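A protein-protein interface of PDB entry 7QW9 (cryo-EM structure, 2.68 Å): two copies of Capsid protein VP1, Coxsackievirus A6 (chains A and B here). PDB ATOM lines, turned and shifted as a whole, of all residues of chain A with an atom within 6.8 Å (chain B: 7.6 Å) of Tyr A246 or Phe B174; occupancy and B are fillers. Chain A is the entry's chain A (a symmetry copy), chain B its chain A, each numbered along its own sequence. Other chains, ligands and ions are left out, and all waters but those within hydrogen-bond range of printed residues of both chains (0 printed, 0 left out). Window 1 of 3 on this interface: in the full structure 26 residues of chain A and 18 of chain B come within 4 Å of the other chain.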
ATOM      1  N   ALA A  82      20.109  13.848   5.252  1.00  0.00           N
ATOM      2  CA  ALA A  82      18.923  13.006   5.479  1.00  0.00           C
ATOM      3  C   ALA A  82      17.748  13.567   4.680  1.00  0.00           C
ATOM      4  O   ALA A  82      17.515  14.767   4.759  1.00  0.00           O
ATOM      5  CB  ALA A  82      18.620  12.927   6.952  1.00  0.00           C
ATOM      6  N   GLY A  83      17.006  12.725   3.961  1.00  0.00           N
ATOM      7  CA  GLY A  83      15.785  13.126   3.239  1.00  0.00           C
ATOM      8  C   GLY A  83      14.650  12.155   3.491  1.00  0.00           C
ATOM      9  O   GLY A  83      14.913  10.978   3.748  1.00  0.00           O
ATOM     10  N   LEU A  84      13.405  12.605   3.397  1.00  0.00           N
ATOM     11  CA  LEU A  84      12.213  11.753   3.626  1.00  0.00           C
ATOM     12  C   LEU A  84      12.183  10.635   2.582  1.00  0.00           C
ATOM     13  O   LEU A  84      12.222  10.946   1.374  1.00  0.00           O
ATOM     14  CB  LEU A  84      10.958  12.614   3.519  1.00  0.00           C
ATOM     15  CG  LEU A  84       9.661  11.917   3.886  1.00  0.00           C
ATOM     16  CD1 LEU A  84       9.690  11.522   5.344  1.00  0.00           C
ATOM     17  CD2 LEU A  84       8.480  12.815   3.599  1.00  0.00           C
ATOM     18  N   VAL A  85      12.136   9.380   3.026  1.00  0.00           N
ATOM     19  CA  VAL A  85      12.094   8.205   2.126  1.00  0.00           C
ATOM     20  C   VAL A  85      10.829   7.404   2.360  1.00  0.00           C
ATOM     21  O   VAL A  85      10.546   6.566   1.502  1.00  0.00           O
ATOM     22  CB  VAL A  85      13.340   7.334   2.282  1.00  0.00           C
ATOM     23  CG1 VAL A  85      14.567   8.067   1.785  1.00  0.00           C
ATOM     24  CG2 VAL A  85      13.552   6.850   3.699  1.00  0.00           C
ATOM     25  N   GLY A  86      10.089   7.647   3.437  1.00  0.00           N
ATOM     26  CA  GLY A  86       8.848   6.901   3.723  1.00  0.00           C
ATOM     27  C   GLY A  86       8.010   7.588   4.777  1.00  0.00           C
ATOM     28  O   GLY A  86       8.598   8.131   5.704  1.00  0.00           O
ATOM     29  N   GLN A 113      14.524  12.906  -3.003  1.00  0.00           N
ATOM     30  CA  GLN A 113      15.591  11.921  -2.691  1.00  0.00           C
ATOM     31  C   GLN A 113      15.766  11.042  -3.921  1.00  0.00           C
ATOM     32  O   GLN A 113      16.911  10.790  -4.295  1.00  0.00           O
ATOM     33  CB  GLN A 113      15.235  11.131  -1.432  1.00  0.00           C
ATOM     34  CG  GLN A 113      16.296  10.142  -0.994  1.00  0.00           C
ATOM     35  CD  GLN A 113      17.488  10.822  -0.376  1.00  0.00           C
ATOM     36  OE1 GLN A 113      18.420  11.237  -1.066  1.00  0.00           O
ATOM     37  NE2 GLN A 113      17.486  10.910   0.941  1.00  0.00           N
ATOM     38  N   GLU A 128      22.087   5.947   7.334  1.00  0.00           N
ATOM     39  CA  GLU A 128      21.603   6.210   8.706  1.00  0.00           C
ATOM     40  C   GLU A 128      20.104   6.540   8.637  1.00  0.00           C
ATOM     41  O   GLU A 128      19.755   7.485   7.961  1.00  0.00           O
ATOM     42  CB  GLU A 128      22.480   7.312   9.268  1.00  0.00           C
ATOM     43  CG  GLU A 128      21.946   7.930  10.531  1.00  0.00           C
ATOM     44  CD  GLU A 128      22.719   9.182  10.927  1.00  0.00           C
ATOM     45  OE1 GLU A 128      23.547   9.103  11.885  1.00  0.00           O
ATOM     46  OE2 GLU A 128      22.508  10.245  10.265  1.00  0.00           O
ATOM     47  N   PHE A 129      19.250   5.789   9.333  1.00  0.00           N
ATOM     48  CA  PHE A 129      17.773   5.909   9.322  1.00  0.00           C
ATOM     49  C   PHE A 129      17.310   6.564  10.613  1.00  0.00           C
ATOM     50  O   PHE A 129      17.619   6.027  11.669  1.00  0.00           O
ATOM     51  CB  PHE A 129      17.124   4.534   9.220  1.00  0.00           C
ATOM     52  CG  PHE A 129      17.079   4.019   7.815  1.00  0.00           C
ATOM     53  CD1 PHE A 129      18.188   3.460   7.231  1.00  0.00           C
ATOM     54  CD2 PHE A 129      15.957   4.186   7.047  1.00  0.00           C
ATOM     55  CE1 PHE A 129      18.156   3.030   5.917  1.00  0.00           C
ATOM     56  CE2 PHE A 129      15.925   3.762   5.735  1.00  0.00           C
ATOM     57  CZ  PHE A 129      17.022   3.183   5.171  1.00  0.00           C
ATOM     58  N   THR A 130      16.538   7.646  10.527  1.00  0.00           N
ATOM     59  CA  THR A 130      15.943   8.351  11.684  1.00  0.00           C
ATOM     60  C   THR A 130      14.432   8.231  11.601  1.00  0.00           C
ATOM     61  O   THR A 130      13.895   8.444  10.524  1.00  0.00           O
ATOM     62  CB  THR A 130      16.368   9.811  11.698  1.00  0.00           C
ATOM     63  OG1 THR A 130      17.760   9.841  11.405  1.00  0.00           O
ATOM     64  CG2 THR A 130      16.116  10.481  13.029  1.00  0.00           C
ATOM     65  N   PHE A 131      13.766   7.938  12.709  1.00  0.00           N
ATOM     66  CA  PHE A 131      12.292   7.810  12.779  1.00  0.00           C
ATOM     67  C   PHE A 131      11.705   8.982  13.575  1.00  0.00           C
ATOM     68  O   PHE A 131      11.629   8.943  14.813  1.00  0.00           O
ATOM     69  CB  PHE A 131      11.943   6.470  13.415  1.00  0.00           C
ATOM     70  CG  PHE A 131      12.480   5.299  12.655  1.00  0.00           C
ATOM     71  CD1 PHE A 131      11.753   4.755  11.631  1.00  0.00           C
ATOM     72  CD2 PHE A 131      13.711   4.762  12.952  1.00  0.00           C
ATOM     73  CE1 PHE A 131      12.241   3.676  10.929  1.00  0.00           C
ATOM     74  CE2 PHE A 131      14.203   3.684  12.240  1.00  0.00           C
ATOM     75  CZ  PHE A 131      13.466   3.153  11.225  1.00  0.00           C
ATOM     76  N   VAL A 132      11.266  10.019  12.883  1.00  0.00           N
ATOM     77  CA  VAL A 132      10.485  11.122  13.494  1.00  0.00           C
ATOM     78  C   VAL A 132       9.049  10.632  13.576  1.00  0.00           C
ATOM     79  O   VAL A 132       8.431  10.527  12.534  1.00  0.00           O
ATOM     80  CB  VAL A 132      10.610  12.393  12.649  1.00  0.00           C
ATOM     81  CG1 VAL A 132       9.798  13.505  13.242  1.00  0.00           C
ATOM     82  CG2 VAL A 132      12.057  12.834  12.499  1.00  0.00           C
ATOM     83  N   PRO A 181      14.296  11.450  18.166  1.00  0.00           N
ATOM     84  CA  PRO A 181      13.977  10.410  17.193  1.00  0.00           C
ATOM     85  C   PRO A 181      14.989   9.268  17.189  1.00  0.00           C
ATOM     86  O   PRO A 181      16.189   9.525  17.237  1.00  0.00           O
ATOM     87  CB  PRO A 181      14.005  11.163  15.856  1.00  0.00           C
ATOM     88  CG  PRO A 181      13.722  12.596  16.244  1.00  0.00           C
ATOM     89  CD  PRO A 181      14.499  12.757  17.533  1.00  0.00           C
ATOM     90  N   GLN A 183      17.654   6.608  15.843  1.00  0.00           N
ATOM     91  CA  GLN A 183      18.540   6.629  14.667  1.00  0.00           C
ATOM     92  C   GLN A 183      19.395   5.388  14.728  1.00  0.00           C
ATOM     93  O   GLN A 183      19.803   5.038  15.825  1.00  0.00           O
ATOM     94  CB  GLN A 183      19.423   7.869  14.700  1.00  0.00           C
ATOM     95  CG  GLN A 183      19.789   8.364  13.318  1.00  0.00           C
ATOM     96  CD  GLN A 183      20.398   9.727  13.435  1.00  0.00           C
ATOM     97  OE1 GLN A 183      19.778  10.734  13.099  1.00  0.00           O
ATOM     98  NE2 GLN A 183      21.621   9.758  13.922  1.00  0.00           N
ATOM     99  N   ARG A 244       7.572   9.346   9.973  1.00  0.00           N
ATOM    100  CA  ARG A 244       8.411   9.873   8.891  1.00  0.00           C
ATOM    101  C   ARG A 244       9.784   9.226   9.021  1.00  0.00           C
ATOM    102  O   ARG A 244      10.470   9.496  10.018  1.00  0.00           O
ATOM    103  CB  ARG A 244       8.465  11.389   8.989  1.00  0.00           C
ATOM    104  CG  ARG A 244       7.163  12.020   8.550  1.00  0.00           C
ATOM    105  CD  ARG A 244       7.166  13.515   8.711  1.00  0.00           C
ATOM    106  NE  ARG A 244       5.849  14.055   8.406  1.00  0.00           N
ATOM    107  CZ  ARG A 244       4.784  13.955   9.193  1.00  0.00           C
ATOM    108  NH1 ARG A 244       4.861  13.342  10.369  1.00  0.00           N
ATOM    109  NH2 ARG A 244       3.640  14.494   8.802  1.00  0.00           N
ATOM    110  N   VAL A 245      10.176   8.427   8.030  1.00  0.00           N
ATOM    111  CA  VAL A 245      11.483   7.738   7.957  1.00  0.00           C
ATOM    112  C   VAL A 245      12.422   8.620   7.153  1.00  0.00           C
ATOM    113  O   VAL A 245      12.050   8.958   6.053  1.00  0.00           O
ATOM    114  CB  VAL A 245      11.303   6.383   7.289  1.00  0.00           C
ATOM    115  CG1 VAL A 245      12.605   5.621   7.263  1.00  0.00           C
ATOM    116  CG2 VAL A 245      10.238   5.577   7.992  1.00  0.00           C
ATOM    117  N   TYR A 246      13.592   8.972   7.692  1.00  0.00           N
ATOM    118  CA  TYR A 246      14.615   9.853   7.072  1.00  0.00           C
ATOM    119  C   TYR A 246      15.906   9.069   6.834  1.00  0.00           C
ATOM    120  O   TYR A 246      16.438   8.496   7.782  1.00  0.00           O
ATOM    121  CB  TYR A 246      14.871  11.042   7.988  1.00  0.00           C
ATOM    122  CG  TYR A 246      13.758  12.031   7.909  1.00  0.00           C
ATOM    123  CD1 TYR A 246      13.696  12.927   6.881  1.00  0.00           C
ATOM    124  CD2 TYR A 246      12.747  12.033   8.822  1.00  0.00           C
ATOM    125  CE1 TYR A 246      12.669  13.838   6.768  1.00  0.00           C
ATOM    126  CE2 TYR A 246      11.701  12.928   8.729  1.00  0.00           C
ATOM    127  CZ  TYR A 246      11.657  13.827   7.692  1.00  0.00           C
ATOM    128  OH  TYR A 246      10.629  14.719   7.569  1.00  0.00           O
ATOM    129  N   MET A 247      16.401   9.039   5.604  1.00  0.00           N
ATOM    130  CA  MET A 247      17.570   8.227   5.245  1.00  0.00           C
ATOM    131  C   MET A 247      18.665   9.205   4.925  1.00  0.00           C
ATOM    132  O   MET A 247      18.434  10.008   4.049  1.00  0.00           O
ATOM    133  CB  MET A 247      17.310   7.370   4.009  1.00  0.00           C
ATOM    134  CG  MET A 247      18.548   6.643   3.540  1.00  0.00           C
ATOM    135  SD  MET A 247      18.300   5.601   2.091  1.00  0.00           S
ATOM    136  CE  MET A 247      18.142   6.820   0.788  1.00  0.00           C
ATOM    137  N   ARG A 248      19.814   9.081   5.567  1.00  0.00           N
ATOM    138  CA  ARG A 248      21.044   9.819   5.226  1.00  0.00           C
ATOM    139  C   ARG A 248      22.076   8.817   4.739  1.00  0.00           C
ATOM    140  O   ARG A 248      22.736   8.202   5.590  1.00  0.00           O
ATOM    141  CB  ARG A 248      21.564  10.531   6.464  1.00  0.00           C
ATOM    142  CG  ARG A 248      22.861  11.281   6.239  1.00  0.00           C
ATOM    143  CD  ARG A 248      23.177  12.153   7.433  1.00  0.00           C
ATOM    144  NE  ARG A 248      24.053  11.473   8.369  1.00  0.00           N
ATOM    145  CZ  ARG A 248      25.349  11.257   8.176  1.00  0.00           C
ATOM    146  NH1 ARG A 248      25.944  11.634   7.056  1.00  0.00           N
ATOM    147  NH2 ARG A 248      26.062  10.651   9.107  1.00  0.00           N
ATOM    148  N   LEU B 144       5.878  18.620  18.071  1.00  0.00           N
ATOM    149  CA  LEU B 144       7.018  18.503  17.125  1.00  0.00           C
ATOM    150  C   LEU B 144       6.988  19.635  16.105  1.00  0.00           C
ATOM    151  O   LEU B 144       5.882  19.948  15.615  1.00  0.00           O
ATOM    152  CB  LEU B 144       6.912  17.163  16.417  1.00  0.00           C
ATOM    153  CG  LEU B 144       8.134  16.775  15.618  1.00  0.00           C
ATOM    154  CD1 LEU B 144       9.355  16.615  16.506  1.00  0.00           C
ATOM    155  CD2 LEU B 144       7.839  15.501  14.885  1.00  0.00           C
ATOM    156  N   LEU B 145       8.138  20.256  15.835  1.00  0.00           N
ATOM    157  CA  LEU B 145       8.275  21.438  14.939  1.00  0.00           C
ATOM    158  C   LEU B 145       9.439  21.204  13.990  1.00  0.00           C
ATOM    159  O   LEU B 145      10.443  20.664  14.450  1.00  0.00           O
ATOM    160  CB  LEU B 145       8.533  22.694  15.767  1.00  0.00           C
ATOM    161  CG  LEU B 145       7.279  23.426  16.202  1.00  0.00           C
ATOM    162  CD1 LEU B 145       6.537  22.650  17.286  1.00  0.00           C
ATOM    163  CD2 LEU B 145       7.640  24.800  16.684  1.00  0.00           C
ATOM    164  N   GLN B 146       9.320  21.628  12.731  1.00  0.00           N
ATOM    165  CA  GLN B 146      10.395  21.477  11.733  1.00  0.00           C
ATOM    166  C   GLN B 146      10.888  22.856  11.341  1.00  0.00           C
ATOM    167  O   GLN B 146      10.099  23.630  10.808  1.00  0.00           O
ATOM    168  CB  GLN B 146       9.902  20.773  10.493  1.00  0.00           C
ATOM    169  CG  GLN B 146      11.013  20.584   9.476  1.00  0.00           C
ATOM    170  CD  GLN B 146      10.544  19.812   8.278  1.00  0.00           C
ATOM    171  OE1 GLN B 146       9.511  19.164   8.306  1.00  0.00           O
ATOM    172  NE2 GLN B 146      11.308  19.885   7.209  1.00  0.00           N
ATOM    173  N   TYR B 147      12.167  23.121  11.563  1.00  0.00           N
ATOM    174  CA  TYR B 147      12.858  24.361  11.191  1.00  0.00           C
ATOM    175  C   TYR B 147      13.679  24.002   9.971  1.00  0.00           C
ATOM    176  O   TYR B 147      14.674  23.290  10.164  1.00  0.00           O
ATOM    177  CB  TYR B 147      13.784  24.787  12.327  1.00  0.00           C
ATOM    178  CG  TYR B 147      13.122  24.955  13.663  1.00  0.00           C
ATOM    179  CD1 TYR B 147      12.965  23.888  14.515  1.00  0.00           C
ATOM    180  CD2 TYR B 147      12.677  26.182  14.079  1.00  0.00           C
ATOM    181  CE1 TYR B 147      12.356  24.019  15.745  1.00  0.00           C
ATOM    182  CE2 TYR B 147      12.073  26.335  15.306  1.00  0.00           C
ATOM    183  CZ  TYR B 147      11.916  25.252  16.140  1.00  0.00           C
ATOM    184  OH  TYR B 147      11.341  25.397  17.356  1.00  0.00           O
ATOM    185  N   MET B 148      13.312  24.480   8.791  1.00  0.00           N
ATOM    186  CA  MET B 148      14.058  24.199   7.553  1.00  0.00           C
ATOM    187  C   MET B 148      14.663  25.478   7.000  1.00  0.00           C
ATOM    188  O   MET B 148      13.895  26.360   6.627  1.00  0.00           O
ATOM    189  CB  MET B 148      13.120  23.621   6.505  1.00  0.00           C
ATOM    190  CG  MET B 148      13.824  23.303   5.213  1.00  0.00           C
ATOM    191  SD  MET B 148      12.719  22.422   4.128  1.00  0.00           S
ATOM    192  CE  MET B 148      11.625  23.741   3.611  1.00  0.00           C
ATOM    193  N   TRP B 165       9.047  20.013   2.198  1.00  0.00           N
ATOM    194  CA  TRP B 165       9.460  19.593   3.565  1.00  0.00           C
ATOM    195  C   TRP B 165      10.128  18.228   3.554  1.00  0.00           C
ATOM    196  O   TRP B 165      10.325  17.695   4.637  1.00  0.00           O
ATOM    197  CB  TRP B 165       8.265  19.523   4.510  1.00  0.00           C
ATOM    198  CG  TRP B 165       7.520  20.795   4.669  1.00  0.00           C
ATOM    199  CD1 TRP B 165       6.316  21.102   4.132  1.00  0.00           C
ATOM    200  CD2 TRP B 165       7.910  21.922   5.451  1.00  0.00           C
ATOM    201  NE1 TRP B 165       5.942  22.361   4.502  1.00  0.00           N
ATOM    202  CE2 TRP B 165       6.895  22.878   5.324  1.00  0.00           C
ATOM    203  CE3 TRP B 165       9.006  22.213   6.255  1.00  0.00           C
ATOM    204  CZ2 TRP B 165       6.954  24.108   5.956  1.00  0.00           C
ATOM    205  CZ3 TRP B 165       9.070  23.435   6.872  1.00  0.00           C
ATOM    206  CH2 TRP B 165       8.058  24.364   6.718  1.00  0.00           C
ATOM    207  N   GLN B 166      10.408  17.639   2.408  1.00  0.00           N
ATOM    208  CA  GLN B 166      11.142  16.354   2.344  1.00  0.00           C
ATOM    209  C   GLN B 166      12.598  16.592   2.726  1.00  0.00           C
ATOM    210  O   GLN B 166      13.158  15.695   3.345  1.00  0.00           O
ATOM    211  CB  GLN B 166      11.002  15.731   0.961  1.00  0.00           C
ATOM    212  CG  GLN B 166       9.590  15.243   0.708  1.00  0.00           C
ATOM    213  CD  GLN B 166       9.311  14.879  -0.724  1.00  0.00           C
ATOM    214  OE1 GLN B 166      10.184  14.874  -1.584  1.00  0.00           O
ATOM    215  NE2 GLN B 166       8.060  14.565  -0.988  1.00  0.00           N
ATOM    216  N   THR B 167      13.168  17.748   2.379  1.00  0.00           N
ATOM    217  CA  THR B 167      14.522  18.210   2.778  1.00  0.00           C
ATOM    218  C   THR B 167      15.563  17.204   2.298  1.00  0.00           C
ATOM    219  O   THR B 167      16.344  16.755   3.139  1.00  0.00           O
ATOM    220  CB  THR B 167      14.682  18.390   4.301  1.00  0.00           C
ATOM    221  OG1 THR B 167      14.730  17.158   5.021  1.00  0.00           O
ATOM    222  CG2 THR B 167      13.571  19.174   4.949  1.00  0.00           C
ATOM    223  N   ALA B 168      15.582  16.814   1.024  1.00  0.00           N
ATOM    224  CA  ALA B 168      16.644  15.919   0.529  1.00  0.00           C
ATOM    225  C   ALA B 168      17.966  16.657   0.701  1.00  0.00           C
ATOM    226  O   ALA B 168      18.934  15.990   1.102  1.00  0.00           O
ATOM    227  CB  ALA B 168      16.424  15.518  -0.897  1.00  0.00           C
ATOM    228  N   SER B 172      17.313  20.902   7.652  1.00  0.00           N
ATOM    229  CA  SER B 172      16.181  21.136   8.571  1.00  0.00           C
ATOM    230  C   SER B 172      16.509  20.609   9.967  1.00  0.00           C
ATOM    231  O   SER B 172      17.428  19.803  10.076  1.00  0.00           O
ATOM    232  CB  SER B 172      14.970  20.503   8.032  1.00  0.00           C
ATOM    233  OG  SER B 172      15.172  19.111   8.022  1.00  0.00           O
ATOM    234  N   ILE B 173      15.770  21.057  10.988  1.00  0.00           N
ATOM    235  CA  ILE B 173      15.950  20.685  12.417  1.00  0.00           C
ATOM    236  C   ILE B 173      14.577  20.308  12.943  1.00  0.00           C
ATOM    237  O   ILE B 173      13.728  21.183  13.016  1.00  0.00           O
ATOM    238  CB  ILE B 173      16.545  21.816  13.263  1.00  0.00           C
ATOM    239  CG1 ILE B 173      17.711  22.535  12.590  1.00  0.00           C
ATOM    240  CG2 ILE B 173      16.976  21.260  14.603  1.00  0.00           C
ATOM    241  CD1 ILE B 173      18.049  23.860  13.232  1.00  0.00           C
ATOM    242  N   PHE B 174      14.386  19.047  13.320  1.00  0.00           N
ATOM    243  CA  PHE B 174      13.203  18.539  14.053  1.00  0.00           C
ATOM    244  C   PHE B 174      13.479  18.640  15.546  1.00  0.00           C
ATOM    245  O   PHE B 174      14.521  18.135  15.978  1.00  0.00           O
ATOM    246  CB  PHE B 174      12.935  17.101  13.650  1.00  0.00           C
ATOM    247  CG  PHE B 174      12.515  16.982  12.217  1.00  0.00           C
ATOM    248  CD1 PHE B 174      13.442  16.816  11.213  1.00  0.00           C
ATOM    249  CD2 PHE B 174      11.188  17.060  11.878  1.00  0.00           C
ATOM    250  CE1 PHE B 174      13.048  16.705   9.893  1.00  0.00           C
ATOM    251  CE2 PHE B 174      10.796  16.925  10.564  1.00  0.00           C
ATOM    252  CZ  PHE B 174      11.727  16.769   9.576  1.00  0.00           C
ATOM    253  N   ALA B 175      12.606  19.299  16.301  1.00  0.00           N
ATOM    254  CA  ALA B 175      12.667  19.365  17.774  1.00  0.00           C
ATOM    255  C   ALA B 175      11.264  19.476  18.319  1.00  0.00           C
ATOM    256  O   ALA B 175      10.431  20.008  17.633  1.00  0.00           O
ATOM    257  CB  ALA B 175      13.466  20.555  18.200  1.00  0.00           C
ATOM    258  N   LYS B 176      11.044  19.002  19.529  1.00  0.00           N
ATOM    259  CA  LYS B 176       9.782  19.207  20.272  1.00  0.00           C
ATOM    260  C   LYS B 176       9.901  20.540  21.004  1.00  0.00           C
ATOM    261  O   LYS B 176      11.019  20.862  21.391  1.00  0.00           O
ATOM    262  CB  LYS B 176       9.566  18.028  21.219  1.00  0.00           C
ATOM    263  CG  LYS B 176       9.229  16.731  20.508  1.00  0.00           C
ATOM    264  CD  LYS B 176       9.487  15.493  21.333  1.00  0.00           C
ATOM    265  CE  LYS B 176      10.893  14.954  21.177  1.00  0.00           C
ATOM    266  NZ  LYS B 176      11.129  14.353  19.841  1.00  0.00           N
ATOM    267  N   ASP B 179      11.759  20.115  24.361  1.00  0.00           N
ATOM    268  CA  ASP B 179      13.238  19.945  24.411  1.00  0.00           C
ATOM    269  C   ASP B 179      13.926  21.282  24.631  1.00  0.00           C
ATOM    270  O   ASP B 179      13.337  22.319  24.361  1.00  0.00           O
ATOM    271  CB  ASP B 179      13.764  19.332  23.112  1.00  0.00           C
ATOM    272  CG  ASP B 179      13.340  17.887  22.907  1.00  0.00           C
ATOM    273  OD1 ASP B 179      12.849  17.261  23.893  1.00  0.00           O
ATOM    274  OD2 ASP B 179      13.496  17.388  21.755  1.00  0.00           O
ATOM    275  N   PRO B 182      16.750  24.315  20.090  1.00  0.00           N
ATOM    276  CA  PRO B 182      17.673  23.895  19.048  1.00  0.00           C
ATOM    277  C   PRO B 182      18.755  24.939  18.746  1.00  0.00           C
ATOM    278  O   PRO B 182      18.437  26.084  18.696  1.00  0.00           O
ATOM    279  CB  PRO B 182      16.796  23.799  17.810  1.00  0.00           C
ATOM    280  CG  PRO B 182      15.409  23.654  18.324  1.00  0.00           C
ATOM    281  CD  PRO B 182      15.371  24.392  19.625  1.00  0.00           C
ATOM    282  N   ARG B 230       7.249  24.794  10.526  1.00  0.00           N
ATOM    283  CA  ARG B 230       5.886  24.213  10.608  1.00  0.00           C
ATOM    284  C   ARG B 230       5.755  23.326  11.830  1.00  0.00           C
ATOM    285  O   ARG B 230       6.787  22.858  12.309  1.00  0.00           O
ATOM    286  CB  ARG B 230       5.602  23.381   9.369  1.00  0.00           C
ATOM    287  CG  ARG B 230       6.506  22.168   9.217  1.00  0.00           C
ATOM    288  CD  ARG B 230       5.805  21.118   8.391  1.00  0.00           C
ATOM    289  NE  ARG B 230       6.625  19.937   8.260  1.00  0.00           N
ATOM    290  CZ  ARG B 230       6.263  18.829   7.635  1.00  0.00           C
ATOM    291  NH1 ARG B 230       5.071  18.739   7.077  1.00  0.00           N
ATOM    292  NH2 ARG B 230       7.100  17.811   7.564  1.00  0.00           N
ATOM    293  N   VAL B 232       4.718  19.710  12.590  1.00  0.00           N
ATOM    294  CA  VAL B 232       4.649  18.485  11.763  1.00  0.00           C
ATOM    295  C   VAL B 232       3.313  17.830  12.086  1.00  0.00           C
ATOM    296  O   VAL B 232       3.309  16.959  12.942  1.00  0.00           O
ATOM    297  CB  VAL B 232       5.835  17.548  12.054  1.00  0.00           C
ATOM    298  CG1 VAL B 232       5.888  16.423  11.043  1.00  0.00           C
ATOM    299  CG2 VAL B 232       7.176  18.264  12.066  1.00  0.00           C
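O of Gln B166 is in hydrogen-bond range of N of Leu A84, at 3.1 Å.
The backbone carbonyl oxygen (O) of Thr B167 sits close to the backbone carbonyl oxygen (O) of Ala A82 (2.8 Å).
No position is printed for both chains.
Of the 10 pairs that touch across the chains among the printed residues, none has its exchanged pair printed and touching as well.
The backbone carbonyl oxygen (O) of Leu B144 is in hydrogen-bond range of the backbone NH (N) of Val B232.
The backbone NH (N) of Met A247 is in hydrogen-bond range of the backbone carbonyl oxygen (O) of Gly A83, at 3.1 Å.
The backbone carbonyl oxygen of Met A247 lies within hydrogen-bond range of the side-chain amide nitrogen of Gln A113, 3.4 Å away.
The backbone carbonyl oxygen (O) of Tyr A246 is in hydrogen-bond range of the backbone NH (N) of Thr A130, at 2.9 Å.
The backbone carbonyl oxygen (O) of Val A132 sits at hydrogen-bond distance from the backbone NH (N) of Arg A244, 2.9 Å away.
Among the printed residues, pairs that only touch across the chains: Gly A83 with Gln B166 (3.7 Å), Gly A83 with Thr B167 (3.7 Å), Gly A83 with Ala B168 (3.99 Å), Gln A113 with Ala B168 (3.9 Å), Val A132 with Leu B144 (3.2 Å), Arg A244 with Val B232 (3.3 Å), Tyr A246 with Gln B166 (3.9 Å) and Tyr A246 with Phe B174 (3.1 Å).
Of the 18 printed residues of chain A, 7 touch a printed residue of chain B.
Printed residues of chain A that touch a printed residue of chain B: Ala A82, Gly A83, Leu A84, Gln A113, Val A132, Arg A244 and Tyr A246.
Hydrophobic or aromatic side chains of chain A within 4 Å of the printed part of chain B: Leu A84, Val A132 and Tyr A246.
Of the 18 printed residues of chain B, 6 touch a printed residue of chain A.
Printed residues of chain B that touch a printed residue of chain A: Leu B144, Gln B166, Thr B167, Ala B168, Phe B174 and Val B232.
Hydrophobic or aromatic side chains of chain B that line the printed part of chain A: Leu B144, Ala B168, Phe B174 and Val B232.
Of the printed residues of chain B, Gly A83 touches Gln B166, Thr B167 and Ala B168.
Of the printed residues of chain B, Val A132 touches Leu B144.
Gln A183 touches none of the printed residues of chain B.
Val A245 touches none of the printed residues of chain B.
Of the printed residues of chain A, Gln B166 touches Gly A83, Leu A84 and Tyr A246.
Of the printed residues of chain A, Phe B174 touches Tyr A246.
The nearest residue of chain B that does not touch Tyr A246 is Trp B165 (4.2 Å).
The nearest residue of chain A that does not touch Phe B174 is Val A132 (4.1 Å).
The nearest printed residue of chain A that does not touch Leu B144 is Arg A244 (5.8 Å).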
